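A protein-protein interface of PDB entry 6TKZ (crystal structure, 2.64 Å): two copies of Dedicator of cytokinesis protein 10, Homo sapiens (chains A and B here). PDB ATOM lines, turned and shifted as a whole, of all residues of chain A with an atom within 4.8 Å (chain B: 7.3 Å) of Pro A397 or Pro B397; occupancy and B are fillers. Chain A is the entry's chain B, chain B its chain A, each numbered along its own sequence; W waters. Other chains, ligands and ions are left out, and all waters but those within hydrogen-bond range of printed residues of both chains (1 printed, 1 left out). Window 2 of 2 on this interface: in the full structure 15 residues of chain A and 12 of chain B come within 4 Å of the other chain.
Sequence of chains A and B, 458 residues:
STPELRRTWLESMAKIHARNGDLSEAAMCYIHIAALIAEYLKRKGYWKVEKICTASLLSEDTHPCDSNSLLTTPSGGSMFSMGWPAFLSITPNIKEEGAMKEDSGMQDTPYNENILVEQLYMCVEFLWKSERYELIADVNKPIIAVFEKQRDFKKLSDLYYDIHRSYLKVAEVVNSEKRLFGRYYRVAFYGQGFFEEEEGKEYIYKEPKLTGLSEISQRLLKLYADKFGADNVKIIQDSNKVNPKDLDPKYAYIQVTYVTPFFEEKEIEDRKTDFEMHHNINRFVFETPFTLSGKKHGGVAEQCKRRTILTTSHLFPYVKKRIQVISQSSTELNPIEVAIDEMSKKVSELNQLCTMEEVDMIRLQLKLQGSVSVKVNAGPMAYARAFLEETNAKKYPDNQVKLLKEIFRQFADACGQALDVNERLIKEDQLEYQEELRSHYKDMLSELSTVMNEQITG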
ATOM      1  N   LYS A 394      19.700   3.393 -17.475  1.00  0.00           N
ATOM      2  CA  LYS A 394      20.170   3.210 -18.844  1.00  0.00           C
ATOM      3  C   LYS A 394      20.109   1.750 -19.290  1.00  0.00           C
ATOM      4  O   LYS A 394      20.306   1.465 -20.479  1.00  0.00           O
ATOM      5  CB  LYS A 394      21.602   3.752 -18.976  1.00  0.00           C
ATOM      6  N   LYS A 395      19.828   0.829 -18.372  1.00  0.00           N
ATOM      7  CA  LYS A 395      19.799  -0.594 -18.663  1.00  0.00           C
ATOM      8  C   LYS A 395      18.393  -1.116 -18.956  1.00  0.00           C
ATOM      9  O   LYS A 395      18.233  -2.327 -19.132  1.00  0.00           O
ATOM     10  CB  LYS A 395      20.416  -1.372 -17.497  1.00  0.00           C
ATOM     11  N   TYR A 396      17.385  -0.246 -19.044  1.00  0.00           N
ATOM     12  CA  TYR A 396      15.991  -0.652 -19.183  1.00  0.00           C
ATOM     13  C   TYR A 396      15.278   0.228 -20.200  1.00  0.00           C
ATOM     14  O   TYR A 396      15.708   1.357 -20.466  1.00  0.00           O
ATOM     15  CB  TYR A 396      15.258  -0.581 -17.832  1.00  0.00           C
ATOM     16  CG  TYR A 396      15.942  -1.344 -16.714  1.00  0.00           C
ATOM     17  CD1 TYR A 396      16.894  -0.722 -15.900  1.00  0.00           C
ATOM     18  CD2 TYR A 396      15.648  -2.684 -16.473  1.00  0.00           C
ATOM     19  CE1 TYR A 396      17.539  -1.425 -14.871  1.00  0.00           C
ATOM     20  CE2 TYR A 396      16.277  -3.392 -15.448  1.00  0.00           C
ATOM     21  CZ  TYR A 396      17.217  -2.755 -14.649  1.00  0.00           C
ATOM     22  OH  TYR A 396      17.837  -3.457 -13.630  1.00  0.00           O
ATOM     23  N   PRO A 397      14.168  -0.255 -20.774  1.00  0.00           N
ATOM     24  CA  PRO A 397      13.446   0.534 -21.790  1.00  0.00           C
ATOM     25  C   PRO A 397      12.920   1.839 -21.227  1.00  0.00           C
ATOM     26  O   PRO A 397      12.332   1.887 -20.145  1.00  0.00           O
ATOM     27  CB  PRO A 397      12.281  -0.371 -22.197  1.00  0.00           C
ATOM     28  CG  PRO A 397      12.691  -1.721 -21.800  1.00  0.00           C
ATOM     29  CD  PRO A 397      13.518  -1.557 -20.558  1.00  0.00           C
ATOM     30  N   ASP A 398      13.094   2.896 -22.014  1.00  0.00           N
ATOM     31  CA  ASP A 398      12.696   4.222 -21.582  1.00  0.00           C
ATOM     32  C   ASP A 398      11.230   4.267 -21.177  1.00  0.00           C
ATOM     33  O   ASP A 398      10.882   4.866 -20.149  1.00  0.00           O
ATOM     34  CB  ASP A 398      12.979   5.213 -22.699  1.00  0.00           C
ATOM     35  CG  ASP A 398      13.190   6.592 -22.189  1.00  0.00           C
ATOM     36  OD1 ASP A 398      14.238   6.827 -21.533  1.00  0.00           O
ATOM     37  OD2 ASP A 398      12.285   7.419 -22.411  1.00  0.00           O
ATOM     38  N   ASN A 399      10.344   3.655 -21.970  1.00  0.00           N
ATOM     39  CA  ASN A 399       8.928   3.693 -21.616  1.00  0.00           C
ATOM     40  C   ASN A 399       8.695   3.059 -20.251  1.00  0.00           C
ATOM     41  O   ASN A 399       7.903   3.570 -19.449  1.00  0.00           O
ATOM     42  CB  ASN A 399       8.073   3.014 -22.695  1.00  0.00           C
ATOM     43  CG  ASN A 399       8.399   1.531 -22.875  1.00  0.00           C
ATOM     44  OD1 ASN A 399       9.565   1.141 -22.916  1.00  0.00           O
ATOM     45  ND2 ASN A 399       7.368   0.707 -23.003  1.00  0.00           N
ATOM     46  N   GLN A 400       9.399   1.964 -19.950  1.00  0.00           N
ATOM     47  CA  GLN A 400       9.178   1.308 -18.669  1.00  0.00           C
ATOM     48  C   GLN A 400       9.763   2.113 -17.517  1.00  0.00           C
ATOM     49  O   GLN A 400       9.151   2.186 -16.444  1.00  0.00           O
ATOM     50  CB  GLN A 400       9.736  -0.116 -18.695  1.00  0.00           C
ATOM     51  CG  GLN A 400       8.723  -1.147 -19.164  1.00  0.00           C
ATOM     52  CD  GLN A 400       9.356  -2.499 -19.420  1.00  0.00           C
ATOM     53  OE1 GLN A 400      10.555  -2.592 -19.673  1.00  0.00           O
ATOM     54  NE2 GLN A 400       8.555  -3.554 -19.363  1.00  0.00           N
ATOM     55  N   VAL A 401      10.928   2.732 -17.716  1.00  0.00           N
ATOM     56  CA  VAL A 401      11.433   3.677 -16.728  1.00  0.00           C
ATOM     57  C   VAL A 401      10.467   4.857 -16.560  1.00  0.00           C
ATOM     58  O   VAL A 401      10.265   5.361 -15.448  1.00  0.00           O
ATOM     59  CB  VAL A 401      12.843   4.143 -17.115  1.00  0.00           C
ATOM     60  CG1 VAL A 401      13.254   5.328 -16.259  1.00  0.00           C
ATOM     61  CG2 VAL A 401      13.849   3.005 -16.973  1.00  0.00           C
ATOM     62  N   ASN B 334      10.254  -6.024 -27.874  1.00  0.00           N
ATOM     63  CA  ASN B 334      10.265  -4.565 -28.152  1.00  0.00           C
ATOM     64  C   ASN B 334      10.748  -4.280 -29.584  1.00  0.00           C
ATOM     65  O   ASN B 334      11.282  -5.162 -30.251  1.00  0.00           O
ATOM     66  CB  ASN B 334      11.188  -3.841 -27.161  1.00  0.00           C
ATOM     67  CG  ASN B 334      10.681  -3.896 -25.751  1.00  0.00           C
ATOM     68  OD1 ASN B 334       9.881  -3.061 -25.330  1.00  0.00           O
ATOM     69  ND2 ASN B 334      11.134  -4.888 -24.999  1.00  0.00           N
ATOM     70  N   ILE B 336      13.445  -2.634 -30.607  1.00  0.00           N
ATOM     71  CA  ILE B 336      14.865  -2.887 -30.791  1.00  0.00           C
ATOM     72  C   ILE B 336      15.154  -4.393 -30.743  1.00  0.00           C
ATOM     73  O   ILE B 336      16.110  -4.868 -31.372  1.00  0.00           O
ATOM     74  CB  ILE B 336      15.703  -2.115 -29.757  1.00  0.00           C
ATOM     75  CG1 ILE B 336      17.166  -2.066 -30.222  1.00  0.00           C
ATOM     76  CG2 ILE B 336      15.582  -2.765 -28.368  1.00  0.00           C
ATOM     77  CD1 ILE B 336      18.089  -1.257 -29.351  1.00  0.00           C
ATOM     78  N   GLU B 337      14.343  -5.163 -30.009  1.00  0.00           N
ATOM     79  CA  GLU B 337      14.540  -6.611 -29.956  1.00  0.00           C
ATOM     80  C   GLU B 337      14.135  -7.260 -31.270  1.00  0.00           C
ATOM     81  O   GLU B 337      14.776  -8.219 -31.706  1.00  0.00           O
ATOM     82  CB  GLU B 337      13.767  -7.225 -28.776  1.00  0.00           C
ATOM     83  CG  GLU B 337      14.478  -7.025 -27.413  1.00  0.00           C
ATOM     84  CD  GLU B 337      13.592  -7.219 -26.167  1.00  0.00           C
ATOM     85  OE1 GLU B 337      12.363  -6.970 -26.211  1.00  0.00           O
ATOM     86  OE2 GLU B 337      14.150  -7.613 -25.125  1.00  0.00           O
ATOM     87  N   ALA B 393      19.407   6.344 -29.594  1.00  0.00           N
ATOM     88  CA  ALA B 393      19.903   5.256 -28.755  1.00  0.00           C
ATOM     89  C   ALA B 393      19.653   5.507 -27.270  1.00  0.00           C
ATOM     90  O   ALA B 393      19.646   4.551 -26.483  1.00  0.00           O
ATOM     91  CB  ALA B 393      21.398   5.014 -28.999  1.00  0.00           C
ATOM     92  N   LYS B 394      19.431   6.761 -26.862  1.00  0.00           N
ATOM     93  CA  LYS B 394      19.246   7.028 -25.437  1.00  0.00           C
ATOM     94  C   LYS B 394      17.957   6.425 -24.881  1.00  0.00           C
ATOM     95  O   LYS B 394      17.823   6.307 -23.657  1.00  0.00           O
ATOM     96  CB  LYS B 394      19.297   8.539 -25.194  1.00  0.00           C
ATOM     97  CG  LYS B 394      20.463   9.219 -25.919  1.00  0.00           C
ATOM     98  CD  LYS B 394      20.837  10.548 -25.280  1.00  0.00           C
ATOM     99  CE  LYS B 394      19.676  11.547 -25.324  1.00  0.00           C
ATOM    100  NZ  LYS B 394      19.798  12.614 -24.271  1.00  0.00           N
ATOM    101  N   LYS B 395      17.038   5.994 -25.741  1.00  0.00           N
ATOM    102  CA  LYS B 395      15.737   5.481 -25.338  1.00  0.00           C
ATOM    103  C   LYS B 395      15.710   3.967 -25.117  1.00  0.00           C
ATOM    104  O   LYS B 395      14.640   3.421 -24.812  1.00  0.00           O
ATOM    105  CB  LYS B 395      14.683   5.851 -26.389  1.00  0.00           C
ATOM    106  CG  LYS B 395      14.473   7.334 -26.529  1.00  0.00           C
ATOM    107  CD  LYS B 395      13.151   7.661 -27.210  1.00  0.00           C
ATOM    108  CE  LYS B 395      13.161   7.250 -28.679  1.00  0.00           C
ATOM    109  NZ  LYS B 395      11.845   7.568 -29.324  1.00  0.00           N
ATOM    110  N   TYR B 396      16.832   3.277 -25.261  1.00  0.00           N
ATOM    111  CA  TYR B 396      16.858   1.824 -25.198  1.00  0.00           C
ATOM    112  C   TYR B 396      18.026   1.379 -24.336  1.00  0.00           C
ATOM    113  O   TYR B 396      18.975   2.137 -24.121  1.00  0.00           O
ATOM    114  CB  TYR B 396      16.967   1.193 -26.601  1.00  0.00           C
ATOM    115  CG  TYR B 396      15.932   1.705 -27.573  1.00  0.00           C
ATOM    116  CD1 TYR B 396      14.683   1.108 -27.684  1.00  0.00           C
ATOM    117  CD2 TYR B 396      16.203   2.809 -28.363  1.00  0.00           C
ATOM    118  CE1 TYR B 396      13.734   1.599 -28.578  1.00  0.00           C
ATOM    119  CE2 TYR B 396      15.275   3.307 -29.245  1.00  0.00           C
ATOM    120  CZ  TYR B 396      14.041   2.708 -29.350  1.00  0.00           C
ATOM    121  OH  TYR B 396      13.127   3.240 -30.243  1.00  0.00           O
ATOM    122  N   PRO B 397      17.964   0.161 -23.806  1.00  0.00           N
ATOM    123  CA  PRO B 397      19.040  -0.327 -22.933  1.00  0.00           C
ATOM    124  C   PRO B 397      20.399  -0.313 -23.623  1.00  0.00           C
ATOM    125  O   PRO B 397      20.518  -0.628 -24.809  1.00  0.00           O
ATOM    126  CB  PRO B 397      18.598  -1.758 -22.602  1.00  0.00           C
ATOM    127  CG  PRO B 397      17.108  -1.730 -22.754  1.00  0.00           C
ATOM    128  CD  PRO B 397      16.815  -0.761 -23.855  1.00  0.00           C
ATOM    129  N   ASP B 398      21.432   0.039 -22.859  1.00  0.00           N
ATOM    130  CA  ASP B 398      22.776   0.090 -23.420  1.00  0.00           C
ATOM    131  C   ASP B 398      23.177  -1.255 -24.010  1.00  0.00           C
ATOM    132  O   ASP B 398      23.738  -1.319 -25.111  1.00  0.00           O
ATOM    133  CB  ASP B 398      23.777   0.537 -22.353  1.00  0.00           C
ATOM    134  CG  ASP B 398      23.712   2.034 -22.102  1.00  0.00           C
ATOM    135  OD1 ASP B 398      22.621   2.620 -22.306  1.00  0.00           O
ATOM    136  OD2 ASP B 398      24.739   2.628 -21.705  1.00  0.00           O
ATOM    137  N   ASN B 399      22.878  -2.344 -23.298  1.00  0.00           N
ATOM    138  CA  ASN B 399      23.310  -3.659 -23.763  1.00  0.00           C
ATOM    139  C   ASN B 399      22.654  -4.021 -25.089  1.00  0.00           C
ATOM    140  O   ASN B 399      23.285  -4.649 -25.946  1.00  0.00           O
ATOM    141  CB  ASN B 399      23.025  -4.726 -22.698  1.00  0.00           C
ATOM    142  CG  ASN B 399      21.552  -4.777 -22.275  1.00  0.00           C
ATOM    143  OD1 ASN B 399      20.847  -5.754 -22.559  1.00  0.00           O
ATOM    144  ND2 ASN B 399      21.082  -3.721 -21.586  1.00  0.00           N
ATOM    145  N   GLN B 400      21.412  -3.613 -25.297  1.00  0.00           N
ATOM    146  CA  GLN B 400      20.787  -3.952 -26.561  1.00  0.00           C
ATOM    147  C   GLN B 400      21.308  -3.076 -27.689  1.00  0.00           C
ATOM    148  O   GLN B 400      21.521  -3.568 -28.809  1.00  0.00           O
ATOM    149  CB  GLN B 400      19.269  -3.888 -26.393  1.00  0.00           C
ATOM    150  CG  GLN B 400      18.830  -5.008 -25.450  1.00  0.00           C
ATOM    151  CD  GLN B 400      17.343  -5.096 -25.228  1.00  0.00           C
ATOM    152  OE1 GLN B 400      16.649  -4.078 -25.141  1.00  0.00           O
ATOM    153  NE2 GLN B 400      16.839  -6.320 -25.122  1.00  0.00           N
ATOM    154  N   VAL B 401      21.589  -1.806 -27.398  1.00  0.00           N
ATOM    155  CA  VAL B 401      22.171  -0.933 -28.413  1.00  0.00           C
ATOM    156  C   VAL B 401      23.542  -1.446 -28.845  1.00  0.00           C
ATOM    157  O   VAL B 401      23.845  -1.508 -30.043  1.00  0.00           O
ATOM    158  CB  VAL B 401      22.239   0.512 -27.898  1.00  0.00           C
ATOM    159  CG1 VAL B 401      23.132   1.353 -28.815  1.00  0.00           C
ATOM    160  CG2 VAL B 401      20.855   1.082 -27.802  1.00  0.00           C
ATOM    161  N   LYS B 402      24.386  -1.849 -27.884  1.00  0.00           N
ATOM    162  CA  LYS B 402      25.699  -2.355 -28.275  1.00  0.00           C
ATOM    163  C   LYS B 402      25.577  -3.685 -29.016  1.00  0.00           C
ATOM    164  O   LYS B 402      26.363  -3.952 -29.934  1.00  0.00           O
ATOM    165  CB  LYS B 402      26.630  -2.480 -27.056  1.00  0.00           C
ATOM    166  CG  LYS B 402      26.675  -1.236 -26.156  1.00  0.00           C
ATOM    167  CD  LYS B 402      26.863   0.081 -26.941  1.00  0.00           C
ATOM    168  CE  LYS B 402      26.621   1.330 -26.052  1.00  0.00           C
ATOM    169  NZ  LYS B 402      26.922   2.632 -26.745  1.00  0.00           N
ATOM    170  N   LEU B 403      24.592  -4.516 -28.658  1.00  0.00           N
ATOM    171  CA  LEU B 403      24.396  -5.768 -29.387  1.00  0.00           C
ATOM    172  C   LEU B 403      23.905  -5.509 -30.804  1.00  0.00           C
ATOM    173  O   LEU B 403      24.392  -6.130 -31.757  1.00  0.00           O
ATOM    174  CB  LEU B 403      23.415  -6.683 -28.658  1.00  0.00           C
ATOM    175  CG  LEU B 403      23.043  -7.929 -29.480  1.00  0.00           C
ATOM    176  CD1 LEU B 403      24.262  -8.819 -29.771  1.00  0.00           C
ATOM    177  CD2 LEU B 403      21.934  -8.733 -28.809  1.00  0.00           C
HETATM  178  O   HOH W   1      11.290   2.893 -25.292  1.00  0.00           O
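Water W1 bridges OD1 of Asn A399 (3.4 Å) and O of Lys B395 (3.4 Å).
Pro B397 touches just these residues of chain A: Lys A394, Lys A395, Tyr A396 and Pro A397.
Printed residues of chain A within 4 Å of Asp B398: Lys A394 (3.0 Å).
Printed residues of chain B within 4 Å of Tyr A396: Pro B397 (3.7 Å).
Glu B337 touches none of the printed residues of chain A.
Asn A399 touches none of the printed residues of chain B.
Lys A394 touches Pro B397, but with the chains exchanged Pro A397 does not touch Lys B394 (7.1 Å).
Lys A395 touches Pro B397, but with the chains exchanged Pro A397 does not touch Lys B395 (4.3 Å).
Pro B397 touches its own counterpart, Pro A397.
Asp A398 touches Lys B395, but with the chains exchanged Lys A395 does not touch Asp B398 (4.5 Å).
8 positions are printed for both chains.
Of the 7 pairs that touch across the chains among the printed residues, 1 has its exchanged pair printed and touching as well.
Among the printed residues, 7 pairs touch across the chains.
Lys A394 touches Tyr B396.
Pro B397 touches Lys A394.
Pro B397 touches Lys A395.
Tyr A396 touches Pro B397.
Pro A397 touches Pro B397.
O of Lys A394 lies within hydrogen-bond range of N of Asp B398.
The backbone carbonyl oxygen of Lys B395 sits close to the backbone NH of Asp A398 (3.2 Å).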
